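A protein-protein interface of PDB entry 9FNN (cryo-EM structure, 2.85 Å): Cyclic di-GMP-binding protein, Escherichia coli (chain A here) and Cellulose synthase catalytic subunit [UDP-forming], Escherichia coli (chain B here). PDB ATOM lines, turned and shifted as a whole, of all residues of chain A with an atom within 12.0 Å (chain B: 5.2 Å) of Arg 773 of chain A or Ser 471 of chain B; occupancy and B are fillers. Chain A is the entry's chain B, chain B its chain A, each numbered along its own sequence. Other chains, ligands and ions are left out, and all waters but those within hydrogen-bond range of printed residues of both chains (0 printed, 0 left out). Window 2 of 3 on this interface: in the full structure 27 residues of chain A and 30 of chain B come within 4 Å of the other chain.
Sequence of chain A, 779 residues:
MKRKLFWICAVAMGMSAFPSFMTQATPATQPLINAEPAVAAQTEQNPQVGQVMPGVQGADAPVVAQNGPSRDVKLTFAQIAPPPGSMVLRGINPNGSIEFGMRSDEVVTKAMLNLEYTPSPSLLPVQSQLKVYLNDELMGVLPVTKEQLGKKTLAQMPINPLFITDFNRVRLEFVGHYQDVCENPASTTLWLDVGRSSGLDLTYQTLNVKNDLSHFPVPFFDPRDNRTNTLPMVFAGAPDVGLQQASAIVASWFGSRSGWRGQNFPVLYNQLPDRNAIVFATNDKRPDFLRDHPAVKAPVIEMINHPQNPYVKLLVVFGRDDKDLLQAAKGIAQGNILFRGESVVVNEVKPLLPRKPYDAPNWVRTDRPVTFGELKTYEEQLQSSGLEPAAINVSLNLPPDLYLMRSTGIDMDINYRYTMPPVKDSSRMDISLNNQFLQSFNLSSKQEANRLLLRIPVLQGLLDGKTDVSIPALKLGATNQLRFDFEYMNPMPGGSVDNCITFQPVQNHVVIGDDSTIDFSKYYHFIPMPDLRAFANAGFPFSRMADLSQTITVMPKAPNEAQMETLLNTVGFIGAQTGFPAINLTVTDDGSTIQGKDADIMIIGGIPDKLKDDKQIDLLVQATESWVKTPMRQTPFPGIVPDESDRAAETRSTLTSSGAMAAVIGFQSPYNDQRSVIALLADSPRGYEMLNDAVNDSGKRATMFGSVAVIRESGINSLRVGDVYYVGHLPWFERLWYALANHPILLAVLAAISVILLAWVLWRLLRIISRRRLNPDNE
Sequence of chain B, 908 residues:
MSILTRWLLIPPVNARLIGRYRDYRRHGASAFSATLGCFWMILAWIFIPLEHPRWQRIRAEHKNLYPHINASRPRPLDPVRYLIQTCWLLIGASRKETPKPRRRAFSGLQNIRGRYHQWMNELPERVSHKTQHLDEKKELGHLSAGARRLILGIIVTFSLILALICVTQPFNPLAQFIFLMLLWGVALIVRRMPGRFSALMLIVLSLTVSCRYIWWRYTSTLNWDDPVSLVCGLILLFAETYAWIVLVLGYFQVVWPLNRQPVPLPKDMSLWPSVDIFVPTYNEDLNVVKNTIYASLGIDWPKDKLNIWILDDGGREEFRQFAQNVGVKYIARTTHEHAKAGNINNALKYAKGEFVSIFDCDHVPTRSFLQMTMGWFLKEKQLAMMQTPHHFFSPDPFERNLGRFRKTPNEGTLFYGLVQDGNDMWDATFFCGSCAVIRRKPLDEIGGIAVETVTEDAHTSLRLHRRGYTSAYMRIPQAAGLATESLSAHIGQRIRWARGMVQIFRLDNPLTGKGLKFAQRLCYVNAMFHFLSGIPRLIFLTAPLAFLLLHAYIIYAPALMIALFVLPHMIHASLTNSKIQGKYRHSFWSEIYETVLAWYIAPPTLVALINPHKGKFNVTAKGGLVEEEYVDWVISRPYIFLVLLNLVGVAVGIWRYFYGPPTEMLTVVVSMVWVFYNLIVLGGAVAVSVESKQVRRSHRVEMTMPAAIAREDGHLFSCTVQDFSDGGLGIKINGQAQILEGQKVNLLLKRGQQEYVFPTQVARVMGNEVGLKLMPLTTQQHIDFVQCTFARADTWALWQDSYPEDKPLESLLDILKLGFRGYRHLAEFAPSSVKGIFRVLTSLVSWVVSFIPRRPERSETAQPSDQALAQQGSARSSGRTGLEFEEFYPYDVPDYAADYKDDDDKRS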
ATOM      1  N   ARG A 764      18.361  -3.803  19.288  1.00  0.00           N
ATOM      2  CA  ARG A 764      19.768  -3.430  19.196  1.00  0.00           C
ATOM      3  C   ARG A 764      20.644  -4.383  20.001  1.00  0.00           C
ATOM      4  O   ARG A 764      21.650  -4.905  19.498  1.00  0.00           O
ATOM      5  CB  ARG A 764      19.953  -1.994  19.685  1.00  0.00           C
ATOM      6  CG  ARG A 764      21.325  -1.410  19.412  1.00  0.00           C
ATOM      7  CD  ARG A 764      21.600  -0.207  20.297  1.00  0.00           C
ATOM      8  NE  ARG A 764      22.150  -0.598  21.588  1.00  0.00           N
ATOM      9  CZ  ARG A 764      23.446  -0.646  21.862  1.00  0.00           C
ATOM     10  NH1 ARG A 764      24.355  -0.313  20.962  1.00  0.00           N
ATOM     11  NH2 ARG A 764      23.841  -1.040  23.069  1.00  0.00           N
ATOM     12  N   LEU A 765      20.268  -4.626  21.260  1.00  0.00           N
ATOM     13  CA  LEU A 765      21.083  -5.476  22.124  1.00  0.00           C
ATOM     14  C   LEU A 765      21.180  -6.892  21.575  1.00  0.00           C
ATOM     15  O   LEU A 765      22.257  -7.504  21.589  1.00  0.00           O
ATOM     16  CB  LEU A 765      20.503  -5.487  23.536  1.00  0.00           C
ATOM     17  CG  LEU A 765      21.229  -6.339  24.571  1.00  0.00           C
ATOM     18  CD1 LEU A 765      22.622  -5.792  24.828  1.00  0.00           C
ATOM     19  CD2 LEU A 765      20.429  -6.402  25.857  1.00  0.00           C
ATOM     20  N   LEU A 766      20.069  -7.428  21.074  1.00  0.00           N
ATOM     21  CA  LEU A 766      20.067  -8.786  20.555  1.00  0.00           C
ATOM     22  C   LEU A 766      20.838  -8.890  19.248  1.00  0.00           C
ATOM     23  O   LEU A 766      21.469  -9.918  18.995  1.00  0.00           O
ATOM     24  CB  LEU A 766      18.634  -9.279  20.382  1.00  0.00           C
ATOM     25  CG  LEU A 766      17.839  -9.474  21.676  1.00  0.00           C
ATOM     26  CD1 LEU A 766      16.406  -9.863  21.371  1.00  0.00           C
ATOM     27  CD2 LEU A 766      18.498 -10.507  22.571  1.00  0.00           C
ATOM     28  N   ARG A 767      20.818  -7.848  18.413  1.00  0.00           N
ATOM     29  CA  ARG A 767      21.684  -7.847  17.237  1.00  0.00           C
ATOM     30  C   ARG A 767      23.152  -7.886  17.638  1.00  0.00           C
ATOM     31  O   ARG A 767      23.948  -8.629  17.047  1.00  0.00           O
ATOM     32  CB  ARG A 767      21.407  -6.621  16.375  1.00  0.00           C
ATOM     33  CG  ARG A 767      20.288  -6.800  15.385  1.00  0.00           C
ATOM     34  CD  ARG A 767      19.968  -5.490  14.706  1.00  0.00           C
ATOM     35  NE  ARG A 767      21.119  -4.933  14.010  1.00  0.00           N
ATOM     36  CZ  ARG A 767      21.347  -5.070  12.711  1.00  0.00           C
ATOM     37  NH1 ARG A 767      20.518  -5.746  11.933  1.00  0.00           N
ATOM     38  NH2 ARG A 767      22.430  -4.512  12.180  1.00  0.00           N
ATOM     39  N   ILE A 768      23.529  -7.092  18.641  1.00  0.00           N
ATOM     40  CA  ILE A 768      24.917  -7.094  19.099  1.00  0.00           C
ATOM     41  C   ILE A 768      25.309  -8.481  19.597  1.00  0.00           C
ATOM     42  O   ILE A 768      26.373  -9.014  19.250  1.00  0.00           O
ATOM     43  CB  ILE A 768      25.128  -6.027  20.188  1.00  0.00           C
ATOM     44  CG1 ILE A 768      24.776  -4.634  19.659  1.00  0.00           C
ATOM     45  CG2 ILE A 768      26.555  -6.063  20.704  1.00  0.00           C
ATOM     46  CD1 ILE A 768      25.443  -4.284  18.358  1.00  0.00           C
ATOM     47  N   ILE A 769      24.448  -9.089  20.416  1.00  0.00           N
ATOM     48  CA  ILE A 769      24.763 -10.397  20.982  1.00  0.00           C
ATOM     49  C   ILE A 769      24.804 -11.461  19.893  1.00  0.00           C
ATOM     50  O   ILE A 769      25.621 -12.384  19.946  1.00  0.00           O
ATOM     51  CB  ILE A 769      23.762 -10.756  22.094  1.00  0.00           C
ATOM     52  CG1 ILE A 769      23.850  -9.747  23.233  1.00  0.00           C
ATOM     53  CG2 ILE A 769      24.025 -12.149  22.625  1.00  0.00           C
ATOM     54  CD1 ILE A 769      22.864 -10.000  24.339  1.00  0.00           C
ATOM     55  N   SER A 770      23.928 -11.357  18.890  1.00  0.00           N
ATOM     56  CA  SER A 770      23.938 -12.320  17.795  1.00  0.00           C
ATOM     57  C   SER A 770      25.222 -12.224  16.986  1.00  0.00           C
ATOM     58  O   SER A 770      25.803 -13.248  16.610  1.00  0.00           O
ATOM     59  CB  SER A 770      22.728 -12.102  16.890  1.00  0.00           C
ATOM     60  OG  SER A 770      22.764 -10.822  16.292  1.00  0.00           O
ATOM     61  N   ARG A 771      25.676 -11.001  16.698  1.00  0.00           N
ATOM     62  CA  ARG A 771      26.927 -10.850  15.962  1.00  0.00           C
ATOM     63  C   ARG A 771      28.110 -11.369  16.768  1.00  0.00           C
ATOM     64  O   ARG A 771      29.005 -12.017  16.214  1.00  0.00           O
ATOM     65  CB  ARG A 771      27.135  -9.390  15.568  1.00  0.00           C
ATOM     66  CG  ARG A 771      26.097  -8.862  14.594  1.00  0.00           C
ATOM     67  CD  ARG A 771      26.461  -7.482  14.069  1.00  0.00           C
ATOM     68  NE  ARG A 771      26.708  -6.524  15.141  1.00  0.00           N
ATOM     69  CZ  ARG A 771      27.914  -6.146  15.545  1.00  0.00           C
ATOM     70  NH1 ARG A 771      29.013  -6.625  14.985  1.00  0.00           N
ATOM     71  NH2 ARG A 771      28.021  -5.265  16.535  1.00  0.00           N
ATOM     72  N   ARG A 772      28.139 -11.099  18.075  1.00  0.00           N
ATOM     73  CA  ARG A 772      29.217 -11.640  18.900  1.00  0.00           C
ATOM     74  C   ARG A 772      29.127 -13.154  19.023  1.00  0.00           C
ATOM     75  O   ARG A 772      30.144 -13.820  19.244  1.00  0.00           O
ATOM     76  CB  ARG A 772      29.199 -11.010  20.292  1.00  0.00           C
ATOM     77  CG  ARG A 772      29.466  -9.520  20.316  1.00  0.00           C
ATOM     78  CD  ARG A 772      29.408  -8.992  21.739  1.00  0.00           C
ATOM     79  NE  ARG A 772      29.578  -7.545  21.798  1.00  0.00           N
ATOM     80  CZ  ARG A 772      29.533  -6.832  22.914  1.00  0.00           C
ATOM     81  NH1 ARG A 772      29.321  -7.401  24.089  1.00  0.00           N
ATOM     82  NH2 ARG A 772      29.702  -5.514  22.849  1.00  0.00           N
ATOM     83  N   ARG A 773      27.924 -13.708  18.898  1.00  0.00           N
ATOM     84  CA  ARG A 773      27.706 -15.135  19.091  1.00  0.00           C
ATOM     85  C   ARG A 773      28.154 -15.945  17.882  1.00  0.00           C
ATOM     86  O   ARG A 773      28.672 -17.056  18.033  1.00  0.00           O
ATOM     87  CB  ARG A 773      26.227 -15.379  19.399  1.00  0.00           C
ATOM     88  CG  ARG A 773      25.827 -16.823  19.538  1.00  0.00           C
ATOM     89  CD  ARG A 773      26.529 -17.494  20.690  1.00  0.00           C
ATOM     90  NE  ARG A 773      26.141 -18.893  20.785  1.00  0.00           N
ATOM     91  CZ  ARG A 773      26.770 -19.795  21.522  1.00  0.00           C
ATOM     92  NH1 ARG A 773      27.830 -19.476  22.247  1.00  0.00           N
ATOM     93  NH2 ARG A 773      26.329 -21.048  21.529  1.00  0.00           N
ATOM     94  N   LEU A 774      27.975 -15.406  16.681  1.00  0.00           N
ATOM     95  CA  LEU A 774      28.337 -16.097  15.452  1.00  0.00           C
ATOM     96  C   LEU A 774      29.788 -15.879  15.050  1.00  0.00           C
ATOM     97  O   LEU A 774      30.196 -16.352  13.985  1.00  0.00           O
ATOM     98  CB  LEU A 774      27.419 -15.659  14.311  1.00  0.00           C
ATOM     99  CG  LEU A 774      25.970 -16.126  14.420  1.00  0.00           C
ATOM    100  CD1 LEU A 774      25.149 -15.607  13.255  1.00  0.00           C
ATOM    101  CD2 LEU A 774      25.915 -17.639  14.487  1.00  0.00           C
ATOM    102  N   ASN A 775      30.568 -15.172  15.861  1.00  0.00           N
ATOM    103  CA  ASN A 775      31.989 -14.985  15.588  1.00  0.00           C
ATOM    104  C   ASN A 775      32.847 -15.649  16.661  1.00  0.00           C
ATOM    105  O   ASN A 775      32.966 -15.150  17.778  1.00  0.00           O
ATOM    106  CB  ASN A 775      32.324 -13.500  15.488  1.00  0.00           C
ATOM    107  CG  ASN A 775      31.682 -12.840  14.288  1.00  0.00           C
ATOM    108  OD1 ASN A 775      30.828 -13.428  13.627  1.00  0.00           O
ATOM    109  ND2 ASN A 775      32.092 -11.611  13.997  1.00  0.00           N
ATOM    110  N   LEU B 258      18.792 -17.728  16.772  1.00  0.00           N
ATOM    111  CA  LEU B 258      20.084 -17.362  16.208  1.00  0.00           C
ATOM    112  C   LEU B 258      20.126 -17.566  14.700  1.00  0.00           C
ATOM    113  O   LEU B 258      20.803 -16.808  13.997  1.00  0.00           O
ATOM    114  CB  LEU B 258      21.191 -18.159  16.892  1.00  0.00           C
ATOM    115  CG  LEU B 258      22.625 -17.843  16.480  1.00  0.00           C
ATOM    116  CD1 LEU B 258      22.902 -16.367  16.625  1.00  0.00           C
ATOM    117  CD2 LEU B 258      23.592 -18.648  17.315  1.00  0.00           C
ATOM    118  N   ARG B 260      21.548 -20.053  12.993  1.00  0.00           N
ATOM    119  CA  ARG B 260      22.909 -20.415  12.629  1.00  0.00           C
ATOM    120  C   ARG B 260      22.934 -21.059  11.250  1.00  0.00           C
ATOM    121  O   ARG B 260      22.042 -21.832  10.890  1.00  0.00           O
ATOM    122  CB  ARG B 260      23.485 -21.381  13.663  1.00  0.00           C
ATOM    123  CG  ARG B 260      24.936 -21.162  14.009  1.00  0.00           C
ATOM    124  CD  ARG B 260      25.423 -22.255  14.935  1.00  0.00           C
ATOM    125  NE  ARG B 260      26.669 -21.906  15.602  1.00  0.00           N
ATOM    126  CZ  ARG B 260      26.758 -21.536  16.872  1.00  0.00           C
ATOM    127  NH1 ARG B 260      25.693 -21.480  17.650  1.00  0.00           N
ATOM    128  NH2 ARG B 260      27.947 -21.219  17.374  1.00  0.00           N
ATOM    129  N   GLU B 380      35.291 -22.940  15.475  1.00  0.00           N
ATOM    130  CA  GLU B 380      35.368 -22.679  16.905  1.00  0.00           C
ATOM    131  C   GLU B 380      36.099 -23.831  17.576  1.00  0.00           C
ATOM    132  O   GLU B 380      35.617 -24.968  17.559  1.00  0.00           O
ATOM    133  CB  GLU B 380      33.979 -22.504  17.512  1.00  0.00           C
ATOM    134  CG  GLU B 380      33.282 -21.216  17.125  1.00  0.00           C
ATOM    135  CD  GLU B 380      32.130 -20.879  18.050  1.00  0.00           C
ATOM    136  OE1 GLU B 380      32.110 -21.397  19.186  1.00  0.00           O
ATOM    137  OE2 GLU B 380      31.246 -20.099  17.643  1.00  0.00           O
ATOM    138  N   LEU B 383      34.075 -25.192  20.700  1.00  0.00           N
ATOM    139  CA  LEU B 383      32.842 -25.940  20.500  1.00  0.00           C
ATOM    140  C   LEU B 383      33.049 -27.396  20.883  1.00  0.00           C
ATOM    141  O   LEU B 383      34.110 -27.975  20.636  1.00  0.00           O
ATOM    142  CB  LEU B 383      32.393 -25.830  19.044  1.00  0.00           C
ATOM    143  CG  LEU B 383      30.897 -25.841  18.732  1.00  0.00           C
ATOM    144  CD1 LEU B 383      30.648 -25.309  17.343  1.00  0.00           C
ATOM    145  CD2 LEU B 383      30.326 -27.231  18.851  1.00  0.00           C
ATOM    146  N   ALA B 384      32.036 -27.986  21.517  1.00  0.00           N
ATOM    147  CA  ALA B 384      32.130 -29.375  21.947  1.00  0.00           C
ATOM    148  C   ALA B 384      30.839 -30.151  21.727  1.00  0.00           C
ATOM    149  O   ALA B 384      30.755 -31.308  22.153  1.00  0.00           O
ATOM    150  CB  ALA B 384      32.530 -29.455  23.419  1.00  0.00           C
ATOM    151  N   MET B 385      29.839 -29.565  21.073  1.00  0.00           N
ATOM    152  CA  MET B 385      28.572 -30.245  20.862  1.00  0.00           C
ATOM    153  C   MET B 385      27.737 -29.528  19.810  1.00  0.00           C
ATOM    154  O   MET B 385      27.556 -28.309  19.877  1.00  0.00           O
ATOM    155  CB  MET B 385      27.804 -30.349  22.181  1.00  0.00           C
ATOM    156  CG  MET B 385      26.584 -31.237  22.128  1.00  0.00           C
ATOM    157  SD  MET B 385      25.099 -30.358  21.617  1.00  0.00           S
ATOM    158  CE  MET B 385      24.097 -31.732  21.078  1.00  0.00           C
ATOM    159  N   ASP B 424      20.271 -21.585  21.272  1.00  0.00           N
ATOM    160  CA  ASP B 424      21.553 -21.427  20.597  1.00  0.00           C
ATOM    161  C   ASP B 424      22.175 -20.069  20.897  1.00  0.00           C
ATOM    162  O   ASP B 424      23.395 -19.964  21.069  1.00  0.00           O
ATOM    163  CB  ASP B 424      21.362 -21.615  19.093  1.00  0.00           C
ATOM    164  CG  ASP B 424      22.660 -21.873  18.367  1.00  0.00           C
ATOM    165  OD1 ASP B 424      23.707 -22.005  19.033  1.00  0.00           O
ATOM    166  OD2 ASP B 424      22.633 -21.945  17.121  1.00  0.00           O
ATOM    167  N   MET B 425      21.356 -19.017  20.954  1.00  0.00           N
ATOM    168  CA  MET B 425      21.893 -17.684  21.200  1.00  0.00           C
ATOM    169  C   MET B 425      22.542 -17.591  22.573  1.00  0.00           C
ATOM    170  O   MET B 425      23.622 -17.006  22.720  1.00  0.00           O
ATOM    171  CB  MET B 425      20.797 -16.635  21.058  1.00  0.00           C
ATOM    172  CG  MET B 425      21.199 -15.285  21.610  1.00  0.00           C
ATOM    173  SD  MET B 425      20.539 -13.926  20.650  1.00  0.00           S
ATOM    174  CE  MET B 425      21.141 -14.393  19.041  1.00  0.00           C
ATOM    175  N   TRP B 426      21.911 -18.168  23.585  1.00  0.00           N
ATOM    176  CA  TRP B 426      22.398 -18.081  24.951  1.00  0.00           C
ATOM    177  C   TRP B 426      23.377 -19.193  25.294  1.00  0.00           C
ATOM    178  O   TRP B 426      23.775 -19.311  26.457  1.00  0.00           O
ATOM    179  CB  TRP B 426      21.219 -18.092  25.924  1.00  0.00           C
ATOM    180  CG  TRP B 426      20.091 -17.220  25.475  1.00  0.00           C
ATOM    181  CD1 TRP B 426      18.868 -17.626  25.042  1.00  0.00           C
ATOM    182  CD2 TRP B 426      20.092 -15.792  25.387  1.00  0.00           C
ATOM    183  NE1 TRP B 426      18.101 -16.541  24.699  1.00  0.00           N
ATOM    184  CE2 TRP B 426      18.833 -15.403  24.903  1.00  0.00           C
ATOM    185  CE3 TRP B 426      21.036 -14.805  25.676  1.00  0.00           C
ATOM    186  CZ2 TRP B 426      18.491 -14.073  24.700  1.00  0.00           C
ATOM    187  CZ3 TRP B 426      20.696 -13.487  25.475  1.00  0.00           C
ATOM    188  CH2 TRP B 426      19.434 -13.131  24.992  1.00  0.00           C
ATOM    189  N   ASP B 427      23.768 -20.004  24.310  1.00  0.00           N
ATOM    190  CA  ASP B 427      24.696 -21.117  24.498  1.00  0.00           C
ATOM    191  C   ASP B 427      24.152 -22.105  25.530  1.00  0.00           C
ATOM    192  O   ASP B 427      24.792 -22.428  26.530  1.00  0.00           O
ATOM    193  CB  ASP B 427      26.089 -20.615  24.886  1.00  0.00           C
ATOM    194  CG  ASP B 427      27.144 -21.693  24.778  1.00  0.00           C
ATOM    195  OD1 ASP B 427      27.331 -22.226  23.665  1.00  0.00           O
ATOM    196  OD2 ASP B 427      27.785 -22.009  25.802  1.00  0.00           O
ATOM    197  N   THR B 429      22.115 -24.944  24.146  1.00  0.00           N
ATOM    198  CA  THR B 429      21.580 -26.028  23.330  1.00  0.00           C
ATOM    199  C   THR B 429      22.080 -27.347  23.901  1.00  0.00           C
ATOM    200  O   THR B 429      23.257 -27.689  23.751  1.00  0.00           O
ATOM    201  CB  THR B 429      22.003 -25.868  21.874  1.00  0.00           C
ATOM    202  OG1 THR B 429      21.526 -24.616  21.373  1.00  0.00           O
ATOM    203  CG2 THR B 429      21.429 -26.990  21.034  1.00  0.00           C
ATOM    204  N   SER B 461      25.665 -32.508  28.429  1.00  0.00           N
ATOM    205  CA  SER B 461      25.721 -31.167  27.857  1.00  0.00           C
ATOM    206  C   SER B 461      25.883 -30.113  28.945  1.00  0.00           C
ATOM    207  O   SER B 461      26.625 -29.137  28.772  1.00  0.00           O
ATOM    208  CB  SER B 461      24.469 -30.898  27.028  1.00  0.00           C
ATOM    209  OG  SER B 461      24.561 -29.647  26.376  1.00  0.00           O
ATOM    210  N   HIS B 465      28.977 -27.484  29.294  1.00  0.00           N
ATOM    211  CA  HIS B 465      28.782 -26.046  29.438  1.00  0.00           C
ATOM    212  C   HIS B 465      29.405 -25.519  30.721  1.00  0.00           C
ATOM    213  O   HIS B 465      29.893 -24.384  30.747  1.00  0.00           O
ATOM    214  CB  HIS B 465      27.296 -25.709  29.399  1.00  0.00           C
ATOM    215  CG  HIS B 465      26.719 -25.684  28.022  1.00  0.00           C
ATOM    216  ND1 HIS B 465      25.495 -26.237  27.721  1.00  0.00           N
ATOM    217  CD2 HIS B 465      27.191 -25.162  26.868  1.00  0.00           C
ATOM    218  CE1 HIS B 465      25.240 -26.062  26.437  1.00  0.00           C
ATOM    219  NE2 HIS B 465      26.254 -25.411  25.897  1.00  0.00           N
ATOM    220  N   TYR B 469      32.978 -25.115  27.638  1.00  0.00           N
ATOM    221  CA  TYR B 469      32.763 -25.406  26.231  1.00  0.00           C
ATOM    222  C   TYR B 469      31.380 -24.951  25.788  1.00  0.00           C
ATOM    223  O   TYR B 469      30.432 -24.913  26.577  1.00  0.00           O
ATOM    224  CB  TYR B 469      32.937 -26.897  25.965  1.00  0.00           C
ATOM    225  CG  TYR B 469      34.267 -27.435  26.427  1.00  0.00           C
ATOM    226  CD1 TYR B 469      35.425 -27.167  25.720  1.00  0.00           C
ATOM    227  CD2 TYR B 469      34.362 -28.210  27.569  1.00  0.00           C
ATOM    228  CE1 TYR B 469      36.640 -27.654  26.140  1.00  0.00           C
ATOM    229  CE2 TYR B 469      35.571 -28.702  27.995  1.00  0.00           C
ATOM    230  CZ  TYR B 469      36.706 -28.421  27.278  1.00  0.00           C
ATOM    231  OH  TYR B 469      37.918 -28.908  27.698  1.00  0.00           O
ATOM    232  N   THR B 470      31.272 -24.609  24.513  1.00  0.00           N
ATOM    233  CA  THR B 470      30.052 -24.068  23.944  1.00  0.00           C
ATOM    234  C   THR B 470      29.257 -25.170  23.248  1.00  0.00           C
ATOM    235  O   THR B 470      29.601 -26.353  23.307  1.00  0.00           O
ATOM    236  CB  THR B 470      30.386 -22.922  22.987  1.00  0.00           C
ATOM    237  OG1 THR B 470      31.148 -23.424  21.884  1.00  0.00           O
ATOM    238  CG2 THR B 470      31.193 -21.858  23.699  1.00  0.00           C
ATOM    239  N   SER B 471      28.172 -24.778  22.587  1.00  0.00           N
ATOM    240  CA  SER B 471      27.326 -25.698  21.842  1.00  0.00           C
ATOM    241  C   SER B 471      26.716 -24.946  20.672  1.00  0.00           C
ATOM    242  O   SER B 471      26.715 -23.714  20.638  1.00  0.00           O
ATOM    243  CB  SER B 471      26.227 -26.300  22.722  1.00  0.00           C
ATOM    244  OG  SER B 471      26.778 -26.971  23.841  1.00  0.00           O
ATOM    245  N   ALA B 472      26.196 -25.698  19.709  1.00  0.00           N
ATOM    246  CA  ALA B 472      25.636 -25.104  18.509  1.00  0.00           C
ATOM    247  C   ALA B 472      24.431 -25.912  18.053  1.00  0.00           C
ATOM    248  O   ALA B 472      24.241 -27.064  18.447  1.00  0.00           O
ATOM    249  CB  ALA B 472      26.674 -25.014  17.385  1.00  0.00           C
ATOM    250  N   TYR B 473      23.609 -25.282  17.218  1.00  0.00           N
ATOM    251  CA  TYR B 473      22.403 -25.900  16.693  1.00  0.00           C
ATOM    252  C   TYR B 473      22.263 -25.570  15.217  1.00  0.00           C
ATOM    253  O   TYR B 473      22.510 -24.435  14.801  1.00  0.00           O
ATOM    254  CB  TYR B 473      21.164 -25.432  17.461  1.00  0.00           C
ATOM    255  CG  TYR B 473      19.884 -26.088  17.018  1.00  0.00           C
ATOM    256  CD1 TYR B 473      19.576 -27.375  17.415  1.00  0.00           C
ATOM    257  CD2 TYR B 473      18.983 -25.421  16.210  1.00  0.00           C
ATOM    258  CE1 TYR B 473      18.416 -27.979  17.016  1.00  0.00           C
ATOM    259  CE2 TYR B 473      17.816 -26.020  15.808  1.00  0.00           C
ATOM    260  CZ  TYR B 473      17.540 -27.299  16.215  1.00  0.00           C
ATOM    261  OH  TYR B 473      16.375 -27.903  15.820  1.00  0.00           O
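Printed residues of chain B within 4 Å of Leu 766 of chain A: Trp 426 (3.7 Å).
Printed residues of chain B within 4 Å of Ser 770 of chain A: Met 425 (3.5 Å).
Arg 771 of chain A touches none of the printed residues of chain B.
Of the printed residues of chain B, Leu 774 of chain A touches Leu 258 and Arg 260.
Of the printed residues of chain A, Arg 260 of chain B touches Arg 773 (3.95 Å) and Leu 774 (3.7 Å).
No residue of chain A comes within 4 Å of Ala 384 of chain B.
Of chain A, only Arg 773 (3.0 Å) comes within 4 Å of Asp 424 of chain B.
Met 425 of chain B touches two residues of chain A.
Of the printed residues of chain A, Trp 426 of chain B touches Leu 766 (3.7 Å).
Of chain A, only Arg 773 comes within 4 Å of Asp 427 of chain B.
Ser 461 of chain B touches none of the printed residues of chain A.
No residue of chain A comes within 4 Å of Ala 472 of chain B.
The nearest residue of chain A that does not touch Ser 471 of chain B is Leu 774 of chain A (8.7 Å).
Printed residues of chain B that touch a printed residue of chain A: Leu 258, Arg 260, Asp 424, Met 425, Trp 426, Asp 427 and Ser 471.
Along chain B the printed residues that touch a printed residue of chain A span positions 258 to 471.
Printed residues of chain A that touch a printed residue of chain B: Leu 766, Ser 770, Arg 773 and Leu 774.
Among the printed residues, 10 pairs touch across the chains.
Among the printed residues, Asp or Glu carboxylates within 4 Å of a Lys or Arg side-chain nitrogen of the other chain: Arg 773 of chain A with Asp 424 of chain B and Arg 773 of chain A with Asp 427 of chain B.
The backbone carbonyl oxygen (O) of Leu 766 of chain A lies within hydrogen-bond range of the side-chain hydroxyl (OG) of Ser 770 of chain A (3.1 Å).
The guanidinium group (NH2) of Arg 260 of chain B lies within salt-bridge range of the side-chain carboxylate (OE2) of Glu 380 of chain B.
The backbone carbonyl oxygen (O) of Arg 767 of chain A is in hydrogen-bond range of the side-chain hydroxyl (OG) of Ser 770 of chain A (2.6 Å).
The backbone NH (N) of Ser 471 of chain B lies within hydrogen-bond range of the side-chain carboxylate (OD1) of Asp 427 of chain B, 2.9 Å away.
N of Tyr 473 of chain B is in hydrogen-bond range of OD2 of Asp 424 of chain B, at 3.5 Å.
The side-chain hydroxyl (OG) of Ser 471 of chain B lies within hydrogen-bond range of a ring nitrogen (NE2) of His 465 of chain B (2.6 Å).
OD1 of Asp 424 of chain B is in salt-bridge range of NH2 of Arg 773 of chain A (3.7 Å).
OD1 of Asp 427 of chain B lies within salt-bridge range of NH2 of Arg 773 of chain A (2.6 Å).
NH2 of Arg 773 of chain A sits at hydrogen-bond distance from O of Ser 471 of chain B, 2.8 Å away.
Leu 766 of chain A touches Trp 426 of chain B.
Met 425 of chain B touches Ser 770 of chain A (CE to CB, 3.5 Å).
CG of Arg 773 of chain A touches CD2 of Leu 258 of chain B (3.6 Å).
Arg 773 of chain A touches Arg 260 of chain B.
Met 425 of chain B touches Arg 773 of chain A.
Leu 258 of chain B touches Leu 774 of chain A.
Leu 774 of chain A touches Arg 260 of chain B.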
